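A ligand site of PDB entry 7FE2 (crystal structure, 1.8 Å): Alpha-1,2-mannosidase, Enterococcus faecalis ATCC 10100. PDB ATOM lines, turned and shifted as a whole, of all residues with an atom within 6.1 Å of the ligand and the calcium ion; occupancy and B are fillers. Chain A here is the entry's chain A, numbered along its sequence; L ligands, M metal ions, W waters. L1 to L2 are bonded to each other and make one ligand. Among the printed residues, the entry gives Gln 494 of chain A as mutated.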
ATOM      1  N   ASN A  22      -0.275   8.705  -0.353  1.00  0.00           N
ATOM      2  CA  ASN A  22       0.973   8.864   0.424  1.00  0.00           C
ATOM      3  C   ASN A  22       1.437  10.310   0.293  1.00  0.00           C
ATOM      4  O   ASN A  22       2.658  10.550   0.229  1.00  0.00           O
ATOM      5  CB  ASN A  22       2.015   7.801  -0.004  1.00  0.00           C
ATOM      6  CG  ASN A  22       2.032   6.621   0.953  1.00  0.00           C
ATOM      7  OD1 ASN A  22       1.840   6.805   2.156  1.00  0.00           O
ATOM      8  ND2 ASN A  22       2.287   5.444   0.447  1.00  0.00           N
ATOM      9  N   PRO A  65       9.749  13.799   0.326  1.00  0.00           N
ATOM     10  CA  PRO A  65       8.974  13.692  -0.904  1.00  0.00           C
ATOM     11  C   PRO A  65       7.967  12.535  -0.890  1.00  0.00           C
ATOM     12  O   PRO A  65       7.159  12.508  -1.763  1.00  0.00           O
ATOM     13  CB  PRO A  65      10.032  13.410  -1.977  1.00  0.00           C
ATOM     14  CG  PRO A  65      11.097  12.603  -1.232  1.00  0.00           C
ATOM     15  CD  PRO A  65      11.055  13.127   0.192  1.00  0.00           C
ATOM     16  N   SER A  66       8.183  11.541  -0.012  1.00  0.00           N
ATOM     17  CA  SER A  66       7.446  10.252   0.037  1.00  0.00           C
ATOM     18  C   SER A  66       7.927   9.529   1.286  1.00  0.00           C
ATOM     19  O   SER A  66       9.015   9.800   1.815  1.00  0.00           O
ATOM     20  CB  SER A  66       7.647   9.417  -1.206  1.00  0.00           C
ATOM     21  OG  SER A  66       8.776   8.585  -1.104  1.00  0.00           O
ATOM     22  N   PRO A  67       7.146   8.585   1.814  1.00  0.00           N
ATOM     23  CA  PRO A  67       7.521   7.900   3.049  1.00  0.00           C
ATOM     24  C   PRO A  67       8.621   6.872   2.781  1.00  0.00           C
ATOM     25  O   PRO A  67       9.291   6.435   3.721  1.00  0.00           O
ATOM     26  CB  PRO A  67       6.200   7.232   3.494  1.00  0.00           C
ATOM     27  CG  PRO A  67       5.422   7.030   2.240  1.00  0.00           C
ATOM     28  CD  PRO A  67       5.843   8.125   1.293  1.00  0.00           C
ATOM     29  N   TRP A  68       8.807   6.512   1.517  1.00  0.00           N
ATOM     30  CA  TRP A  68       9.819   5.547   1.056  1.00  0.00           C
ATOM     31  C   TRP A  68      11.209   6.192   1.041  1.00  0.00           C
ATOM     32  O   TRP A  68      12.195   5.501   1.300  1.00  0.00           O
ATOM     33  CB  TRP A  68       9.421   5.011  -0.327  1.00  0.00           C
ATOM     34  CG  TRP A  68       7.992   4.541  -0.334  1.00  0.00           C
ATOM     35  CD1 TRP A  68       6.967   5.159  -0.991  1.00  0.00           C
ATOM     36  CD2 TRP A  68       7.392   3.528   0.489  1.00  0.00           C
ATOM     37  NE1 TRP A  68       5.765   4.549  -0.687  1.00  0.00           N
ATOM     38  CE2 TRP A  68       5.987   3.552   0.226  1.00  0.00           C
ATOM     39  CE3 TRP A  68       7.877   2.545   1.344  1.00  0.00           C
ATOM     40  CZ2 TRP A  68       5.090   2.679   0.819  1.00  0.00           C
ATOM     41  CZ3 TRP A  68       6.987   1.650   1.898  1.00  0.00           C
ATOM     42  CH2 TRP A  68       5.613   1.735   1.674  1.00  0.00           C
ATOM     43  N   MET A  69      11.280   7.451   0.663  1.00  0.00           N
ATOM     44  CA  MET A  69      12.578   8.206   0.611  1.00  0.00           C
ATOM     45  C   MET A  69      12.885   8.710   2.015  1.00  0.00           C
ATOM     46  O   MET A  69      14.059   8.897   2.326  1.00  0.00           O
ATOM     47  CB  MET A  69      12.515   9.383  -0.376  1.00  0.00           C
ATOM     48  CG  MET A  69      12.226   8.981  -1.836  1.00  0.00           C
ATOM     49  SD  MET A  69      13.181   7.552  -2.415  1.00  0.00           S
ATOM     50  CE  MET A  69      14.766   8.341  -2.247  1.00  0.00           C
ATOM     51  N   GLY A 310      11.778  11.543  -8.482  1.00  0.00           N
ATOM     52  CA  GLY A 310      12.124  10.275  -9.115  1.00  0.00           C
ATOM     53  C   GLY A 310      11.602  10.276 -10.536  1.00  0.00           C
ATOM     54  O   GLY A 310      10.354  10.122 -10.730  1.00  0.00           O
ATOM     55  N   TRP A 312      11.509   8.117 -12.848  1.00  0.00           N
ATOM     56  CA  TRP A 312      10.672   6.910 -13.107  1.00  0.00           C
ATOM     57  C   TRP A 312       9.183   7.277 -12.983  1.00  0.00           C
ATOM     58  O   TRP A 312       8.386   6.773 -13.772  1.00  0.00           O
ATOM     59  CB  TRP A 312      11.066   5.784 -12.144  1.00  0.00           C
ATOM     60  CG  TRP A 312      10.487   4.419 -12.392  1.00  0.00           C
ATOM     61  CD1 TRP A 312      11.046   3.443 -13.175  1.00  0.00           C
ATOM     62  CD2 TRP A 312       9.310   3.841 -11.800  1.00  0.00           C
ATOM     63  NE1 TRP A 312      10.276   2.304 -13.132  1.00  0.00           N
ATOM     64  CE2 TRP A 312       9.217   2.512 -12.279  1.00  0.00           C
ATOM     65  CE3 TRP A 312       8.323   4.297 -10.921  1.00  0.00           C
ATOM     66  CZ2 TRP A 312       8.172   1.651 -11.920  1.00  0.00           C
ATOM     67  CZ3 TRP A 312       7.285   3.455 -10.562  1.00  0.00           C
ATOM     68  CH2 TRP A 312       7.219   2.149 -11.054  1.00  0.00           C
ATOM     69  N   ASP A 313       8.832   8.116 -12.028  1.00  0.00           N
ATOM     70  CA  ASP A 313       7.464   8.636 -11.806  1.00  0.00           C
ATOM     71  C   ASP A 313       7.155   9.887 -12.671  1.00  0.00           C
ATOM     72  O   ASP A 313       6.144   9.893 -13.369  1.00  0.00           O
ATOM     73  CB  ASP A 313       7.275   9.063 -10.344  1.00  0.00           C
ATOM     74  CG  ASP A 313       7.570   8.002  -9.309  1.00  0.00           C
ATOM     75  OD1 ASP A 313       7.132   6.861  -9.523  1.00  0.00           O
ATOM     76  OD2 ASP A 313       8.215   8.367  -8.243  1.00  0.00           O
ATOM     77  N   TRP A 350      16.979   9.591  -8.852  1.00  0.00           N
ATOM     78  CA  TRP A 350      16.061   9.861  -7.711  1.00  0.00           C
ATOM     79  C   TRP A 350      16.777  10.835  -6.774  1.00  0.00           C
ATOM     80  O   TRP A 350      17.651  10.396  -6.012  1.00  0.00           O
ATOM     81  CB  TRP A 350      15.607   8.586  -6.977  1.00  0.00           C
ATOM     82  CG  TRP A 350      14.139   8.521  -6.672  1.00  0.00           C
ATOM     83  CD1 TRP A 350      13.241   7.603  -7.146  1.00  0.00           C
ATOM     84  CD2 TRP A 350      13.355   9.464  -5.933  1.00  0.00           C
ATOM     85  NE1 TRP A 350      11.975   7.883  -6.708  1.00  0.00           N
ATOM     86  CE2 TRP A 350      12.008   9.031  -5.987  1.00  0.00           C
ATOM     87  CE3 TRP A 350      13.643  10.661  -5.276  1.00  0.00           C
ATOM     88  CZ2 TRP A 350      10.967   9.745  -5.393  1.00  0.00           C
ATOM     89  CZ3 TRP A 350      12.620  11.357  -4.685  1.00  0.00           C
ATOM     90  CH2 TRP A 350      11.289  10.919  -4.753  1.00  0.00           C
ATOM     91  N   LEU A 358      17.150   4.970  -6.593  1.00  0.00           N
ATOM     92  CA  LEU A 358      16.024   4.019  -6.420  1.00  0.00           C
ATOM     93  C   LEU A 358      15.202   3.996  -7.732  1.00  0.00           C
ATOM     94  O   LEU A 358      15.164   5.014  -8.465  1.00  0.00           O
ATOM     95  CB  LEU A 358      15.187   4.416  -5.194  1.00  0.00           C
ATOM     96  CG  LEU A 358      14.075   3.438  -4.785  1.00  0.00           C
ATOM     97  CD1 LEU A 358      14.597   2.341  -3.850  1.00  0.00           C
ATOM     98  CD2 LEU A 358      12.921   4.189  -4.111  1.00  0.00           C
ATOM     99  N   MET A 359      14.645   2.817  -8.022  1.00  0.00           N
ATOM    100  CA  MET A 359      13.747   2.484  -9.172  1.00  0.00           C
ATOM    101  C   MET A 359      14.600   2.166 -10.389  1.00  0.00           C
ATOM    102  O   MET A 359      15.743   2.640 -10.518  1.00  0.00           O
ATOM    103  CB  MET A 359      12.730   3.594  -9.495  1.00  0.00           C
ATOM    104  CG  MET A 359      11.823   3.966  -8.316  1.00  0.00           C
ATOM    105  SD  MET A 359      11.170   2.470  -7.456  1.00  0.00           S
ATOM    106  CE  MET A 359      10.011   1.809  -8.666  1.00  0.00           C
ATOM    107  N   GLN A 494       7.487  -4.012  -8.970  1.00  0.00           N
ATOM    108  CA  GLN A 494       6.196  -3.536  -8.410  1.00  0.00           C
ATOM    109  C   GLN A 494       5.071  -3.922  -9.375  1.00  0.00           C
ATOM    110  O   GLN A 494       4.189  -3.078  -9.607  1.00  0.00           O
ATOM    111  CB  GLN A 494       6.227  -2.025  -8.158  1.00  0.00           C
ATOM    112  CG  GLN A 494       7.465  -1.607  -7.367  1.00  0.00           C
ATOM    113  CD  GLN A 494       7.457  -0.165  -6.930  1.00  0.00           C
ATOM    114  OE1 GLN A 494       6.636   0.655  -7.373  1.00  0.00           O
ATOM    115  NE2 GLN A 494       8.392   0.145  -6.045  1.00  0.00           N
ATOM    116  N   TYR A 540       8.274 -11.319  -3.957  1.00  0.00           N
ATOM    117  CA  TYR A 540       8.479 -10.470  -2.758  1.00  0.00           C
ATOM    118  C   TYR A 540       8.537 -11.328  -1.481  1.00  0.00           C
ATOM    119  O   TYR A 540       9.365 -11.001  -0.575  1.00  0.00           O
ATOM    120  CB  TYR A 540       7.401  -9.377  -2.693  1.00  0.00           C
ATOM    121  CG  TYR A 540       7.628  -8.232  -3.657  1.00  0.00           C
ATOM    122  CD1 TYR A 540       8.371  -7.114  -3.287  1.00  0.00           C
ATOM    123  CD2 TYR A 540       7.077  -8.238  -4.938  1.00  0.00           C
ATOM    124  CE1 TYR A 540       8.567  -6.046  -4.169  1.00  0.00           C
ATOM    125  CE2 TYR A 540       7.249  -7.172  -5.819  1.00  0.00           C
ATOM    126  CZ  TYR A 540       8.023  -6.087  -5.443  1.00  0.00           C
ATOM    127  OH  TYR A 540       8.204  -5.037  -6.308  1.00  0.00           O
ATOM    128  N   ILE A 544       2.572  -6.469  -0.807  1.00  0.00           N
ATOM    129  CA  ILE A 544       2.991  -5.049  -0.726  1.00  0.00           C
ATOM    130  C   ILE A 544       1.803  -4.171  -1.128  1.00  0.00           C
ATOM    131  O   ILE A 544       0.868  -4.672  -1.810  1.00  0.00           O
ATOM    132  CB  ILE A 544       4.209  -4.780  -1.628  1.00  0.00           C
ATOM    133  CG1 ILE A 544       3.879  -4.974  -3.104  1.00  0.00           C
ATOM    134  CG2 ILE A 544       5.395  -5.596  -1.168  1.00  0.00           C
ATOM    135  CD1 ILE A 544       5.040  -4.618  -4.037  1.00  0.00           C
ATOM    136  N   HIS A 545       1.827  -2.944  -0.688  1.00  0.00           N
ATOM    137  CA  HIS A 545       0.677  -2.016  -0.842  1.00  0.00           C
ATOM    138  C   HIS A 545       0.252  -1.920  -2.320  1.00  0.00           C
ATOM    139  O   HIS A 545      -0.961  -1.809  -2.547  1.00  0.00           O
ATOM    140  CB  HIS A 545       0.961  -0.683  -0.135  1.00  0.00           C
ATOM    141  CG  HIS A 545       1.899   0.223  -0.845  1.00  0.00           C
ATOM    142  ND1 HIS A 545       1.457   1.233  -1.696  1.00  0.00           N
ATOM    143  CD2 HIS A 545       3.251   0.294  -0.829  1.00  0.00           C
ATOM    144  CE1 HIS A 545       2.511   1.944  -2.101  1.00  0.00           C
ATOM    145  NE2 HIS A 545       3.611   1.362  -1.635  1.00  0.00           N
ATOM    146  N   GLU A 546       1.175  -1.934  -3.301  1.00  0.00           N
ATOM    147  CA  GLU A 546       0.775  -1.827  -4.749  1.00  0.00           C
ATOM    148  C   GLU A 546      -0.130  -2.991  -5.158  1.00  0.00           C
ATOM    149  O   GLU A 546      -0.985  -2.810  -6.006  1.00  0.00           O
ATOM    150  CB  GLU A 546       1.976  -1.774  -5.668  1.00  0.00           C
ATOM    151  CG  GLU A 546       2.718  -0.427  -5.624  1.00  0.00           C
ATOM    152  CD  GLU A 546       3.833  -0.306  -4.604  1.00  0.00           C
ATOM    153  OE1 GLU A 546       4.618   0.702  -4.714  1.00  0.00           O
ATOM    154  OE2 GLU A 546       3.970  -1.227  -3.744  1.00  0.00           O
ATOM    155  N   SER A 561      -3.127   2.340  -9.693  1.00  0.00           N
ATOM    156  CA  SER A 561      -2.448   2.715  -8.430  1.00  0.00           C
ATOM    157  C   SER A 561      -0.927   2.915  -8.608  1.00  0.00           C
ATOM    158  O   SER A 561      -0.285   3.458  -7.669  1.00  0.00           O
ATOM    159  CB  SER A 561      -2.713   1.634  -7.379  1.00  0.00           C
ATOM    160  OG  SER A 561      -2.416   0.358  -7.934  1.00  0.00           O
ATOM    161  N   ASN A 562      -0.341   2.498  -9.727  1.00  0.00           N
ATOM    162  CA  ASN A 562       1.114   2.595  -9.922  1.00  0.00           C
ATOM    163  C   ASN A 562       1.427   2.986 -11.372  1.00  0.00           C
ATOM    164  O   ASN A 562       0.655   2.650 -12.308  1.00  0.00           O
ATOM    165  CB  ASN A 562       1.803   1.281  -9.504  1.00  0.00           C
ATOM    166  CG  ASN A 562       3.271   1.434  -9.179  1.00  0.00           C
ATOM    167  OD1 ASN A 562       3.723   2.520  -8.835  1.00  0.00           O
ATOM    168  ND2 ASN A 562       4.002   0.328  -9.230  1.00  0.00           N
ATOM    169  N   GLN A 563       2.584   3.617 -11.555  1.00  0.00           N
ATOM    170  CA  GLN A 563       3.036   4.226 -12.840  1.00  0.00           C
ATOM    171  C   GLN A 563       3.046   3.254 -14.006  1.00  0.00           C
ATOM    172  O   GLN A 563       2.729   3.688 -15.117  1.00  0.00           O
ATOM    173  CB  GLN A 563       4.418   4.865 -12.685  1.00  0.00           C
ATOM    174  CG  GLN A 563       4.341   6.251 -12.086  1.00  0.00           C
ATOM    175  CD  GLN A 563       4.104   6.182 -10.605  1.00  0.00           C
ATOM    176  OE1 GLN A 563       4.335   5.163  -9.967  1.00  0.00           O
ATOM    177  NE2 GLN A 563       3.635   7.286 -10.048  1.00  0.00           N
ATOM    178  N   PRO A 564       3.436   1.975 -13.852  1.00  0.00           N
ATOM    179  CA  PRO A 564       3.531   1.046 -14.987  1.00  0.00           C
ATOM    180  C   PRO A 564       2.254   0.900 -15.820  1.00  0.00           C
ATOM    181  O   PRO A 564       2.418   0.758 -17.028  1.00  0.00           O
ATOM    182  CB  PRO A 564       3.941  -0.295 -14.354  1.00  0.00           C
ATOM    183  CG  PRO A 564       4.637   0.128 -13.089  1.00  0.00           C
ATOM    184  CD  PRO A 564       3.847   1.319 -12.594  1.00  0.00           C
ATOM    185  N   ASP A 602       0.033   5.743  -4.782  1.00  0.00           N
ATOM    186  CA  ASP A 602       1.033   6.790  -4.453  1.00  0.00           C
ATOM    187  C   ASP A 602       1.003   7.906  -5.517  1.00  0.00           C
ATOM    188  O   ASP A 602       1.030   7.612  -6.732  1.00  0.00           O
ATOM    189  CB  ASP A 602       2.439   6.242  -4.365  1.00  0.00           C
ATOM    190  CG  ASP A 602       2.716   5.464  -3.094  1.00  0.00           C
ATOM    191  OD1 ASP A 602       1.775   5.131  -2.324  1.00  0.00           O
ATOM    192  OD2 ASP A 602       3.863   5.227  -2.881  1.00  0.00           O
ATOM    193  N   ASP A 604       3.199  10.264  -5.866  1.00  0.00           N
ATOM    194  CA  ASP A 604       4.611  10.392  -6.384  1.00  0.00           C
ATOM    195  C   ASP A 604       4.897  11.767  -7.044  1.00  0.00           C
ATOM    196  O   ASP A 604       5.234  11.819  -8.266  1.00  0.00           O
ATOM    197  CB  ASP A 604       4.882   9.251  -7.341  1.00  0.00           C
ATOM    198  CG  ASP A 604       4.907   7.880  -6.675  1.00  0.00           C
ATOM    199  OD1 ASP A 604       5.547   7.756  -5.605  1.00  0.00           O
ATOM    200  OD2 ASP A 604       4.247   6.963  -7.217  1.00  0.00           O
ATOM    201  N   ASN A 605       4.932  12.836  -6.238  1.00  0.00           N
ATOM    202  CA  ASN A 605       5.556  14.147  -6.562  1.00  0.00           C
ATOM    203  C   ASN A 605       5.013  14.705  -7.896  1.00  0.00           C
ATOM    204  O   ASN A 605       5.819  15.154  -8.731  1.00  0.00           O
ATOM    205  CB  ASN A 605       7.070  13.937  -6.583  1.00  0.00           C
ATOM    206  CG  ASN A 605       7.513  13.238  -5.330  1.00  0.00           C
ATOM    207  OD1 ASN A 605       7.945  12.091  -5.367  1.00  0.00           O
ATOM    208  ND2 ASN A 605       7.364  13.900  -4.200  1.00  0.00           N
HETATM  209  C1  LIG L   1       9.435   1.393  -2.342  1.00  0.00           C
HETATM  210  C2  LIG L   1       8.164   2.099  -2.760  1.00  0.00           C
HETATM  211  C3  LIG L   1       6.984   1.250  -2.294  1.00  0.00           C
HETATM  212  C4  LIG L   1       7.088  -0.206  -2.724  1.00  0.00           C
HETATM  213  C5  LIG L   1       8.477  -0.765  -2.501  1.00  0.00           C
HETATM  214  C6  LIG L   1       8.690  -2.076  -3.237  1.00  0.00           C
HETATM  215  O1  LIG L   1      10.570   2.170  -2.743  1.00  0.00           O
HETATM  216  O2  LIG L   1       8.087   2.184  -4.195  1.00  0.00           O
HETATM  217  O3  LIG L   1       5.785   1.828  -2.800  1.00  0.00           O
HETATM  218  O4  LIG L   1       6.085  -0.999  -2.085  1.00  0.00           O
HETATM  219  O5  LIG L   1       9.430   0.137  -3.009  1.00  0.00           O
HETATM  220  O6  LIG L   1       9.548  -2.904  -2.464  1.00  0.00           O
HETATM  221  C1  LG2 L   2       7.944   3.468  -4.802  1.00  0.00           C
HETATM  222  C2  LG2 L   2       7.564   3.496  -6.310  1.00  0.00           C
HETATM  223  C3  LG2 L   2       7.943   4.817  -6.992  1.00  0.00           C
HETATM  224  C4  LG2 L   2       8.650   5.892  -6.102  1.00  0.00           C
HETATM  225  C5  LG2 L   2       9.455   5.341  -4.912  1.00  0.00           C
HETATM  226  C6  LG2 L   2      10.014   6.359  -3.924  1.00  0.00           C
HETATM  227  O1  LG2 L   2       6.160   3.236  -6.663  1.00  0.00           O
HETATM  228  O2  LG2 L   2       6.657   5.132  -7.583  1.00  0.00           O
HETATM  229  O3  LG2 L   2       9.525   6.688  -6.923  1.00  0.00           O
HETATM  230  O4  LG2 L   2       8.515   4.604  -4.156  1.00  0.00           O
HETATM  231  O5  LG2 L   2       9.001   7.258  -3.413  1.00  0.00           O
HETATM  232 CA    CA M   1       4.356   4.550  -7.496  1.00  0.00          CA
HETATM  233  O   HOH W   1       5.945  -1.961   0.422  1.00  0.00           O
HETATM  234  O   HOH W   2       3.534   3.042  -5.760  1.00  0.00           O
HETATM  235  O   HOH W   3       1.872   5.183  -7.614  1.00  0.00           O
HETATM  236  O   HOH W   4       7.690   9.175  -4.811  1.00  0.00           O
HETATM  237  O   HOH W   5       5.625   5.292  -5.015  1.00  0.00           O
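The side-chain carboxylate (OE1) of Glu 546 is in hydrogen-bond range of an oxygen (O3) of LIG L1. OG of Ser 66 is in hydrogen-bond range of O5 of LG2 L2 (2.7 Å). The indole nitrogen of Trp 350 is in hydrogen-bond range of an oxygen (O3) of LG2 L2 (2.7 Å). O3 of LIG L1 lies within hydrogen-bond range of NE1 of Trp 68, 3.4 Å away. An oxygen (O3) of LIG L1 lies within hydrogen-bond range of a ring nitrogen (NE2) of His 545. The side-chain amide nitrogen (NE2) of Gln 494 is in hydrogen-bond range of an oxygen (O2) of LIG L1. An oxygen (O3) of LG2 L2 lies within hydrogen-bond range of the side-chain carboxylate (OD2) of Asp 313 (2.5 Å).
NE1 of Trp 68 lies within hydrogen-bond range of OD2 of Asp 602 (3.0 Å). OG of Ser 66 lies within hydrogen-bond range of N of Met 69 (3.3 Å). The side-chain hydroxyl (OG) of Ser 66 lies close to the backbone NH (N) of Trp 68 (3.3 Å). N of Gln 494 lies within hydrogen-bond range of OH of Tyr 540 (2.9 Å). The side-chain amide nitrogen (ND2) of Asn 22 is in hydrogen-bond range of the side-chain carboxylate (OD1) of Asp 602 (2.8 Å). The side-chain carboxylate of Glu 546 lies close to the side-chain amide oxygen of Gln 494 (3.3 Å). The side-chain amide nitrogen (ND2) of Asn 562 sits at hydrogen-bond distance from the side-chain amide oxygen (OE1) of Gln 494 (3.2 Å). The side-chain amide oxygen (OE1) of Gln 563 sits close to the side-chain carboxylate (OD1) of Asp 313, at 3.3 Å.
Met 69 touches the ligand. CZ3 of Trp 312 touches O2 of LG2 L2, at 3.5 Å. Leu 358 touches the ligand. CE of Met 359 touches C2 of LG2 L2 (3.8 Å). CE1 of Tyr 540 touches O6 of LIG L1, at 3.7 Å. Asp 602 touches the ligand. Hydrophobic or aromatic side chains that line the ligand: Trp 68, Met 69, Trp 312, Trp 350, Leu 358, Met 359, Tyr 540 and His 545. 16 residues have an atom within 4 Å of the ligand: Ser 66, Trp 68, Met 69, Trp 312, Asp 313, Trp 350, Leu 358, Met 359, Gln 494, Tyr 540, His 545, Glu 546, Asn 562, Gln 563, Asp 602 and Asp 604.
Three residues have an atom within 4 Å of the calcium ion: Asn 562, Gln 563 and Asp 604. Along chain A the residues within 4 Å of the calcium ion span positions 562 to 604.
The calcium ion is bound by an oxygen (O2) of LG2 L2. The calcium ion is bound by O1 of LG2 L2, at 2.4 Å. The calcium ion is bound by OD2 of Asp 604, at 2.4 Å. The calcium ion is bound by water W2, 2.4 Å away. The side-chain amide oxygen (OD1) of Asn 562 binds the calcium ion, at 2.5 Å. OE1 of Gln 563 binds the calcium ion (2.5 Å). The calcium ion is bound by water W3, 2.6 Å away. Water W5 is bound to the calcium ion (2.9 Å).
Water W3 lies within hydrogen-bond range of the backbone carbonyl oxygen (O) of Asp 602 and the backbone carbonyl oxygen (O) of Ser 561. Water W4 lies within hydrogen-bond range of the side-chain carboxylate (OD1) of Asp 604, an oxygen (O5) of LG2 L2 and the side-chain amide oxygen (OD1) of Asn 605.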
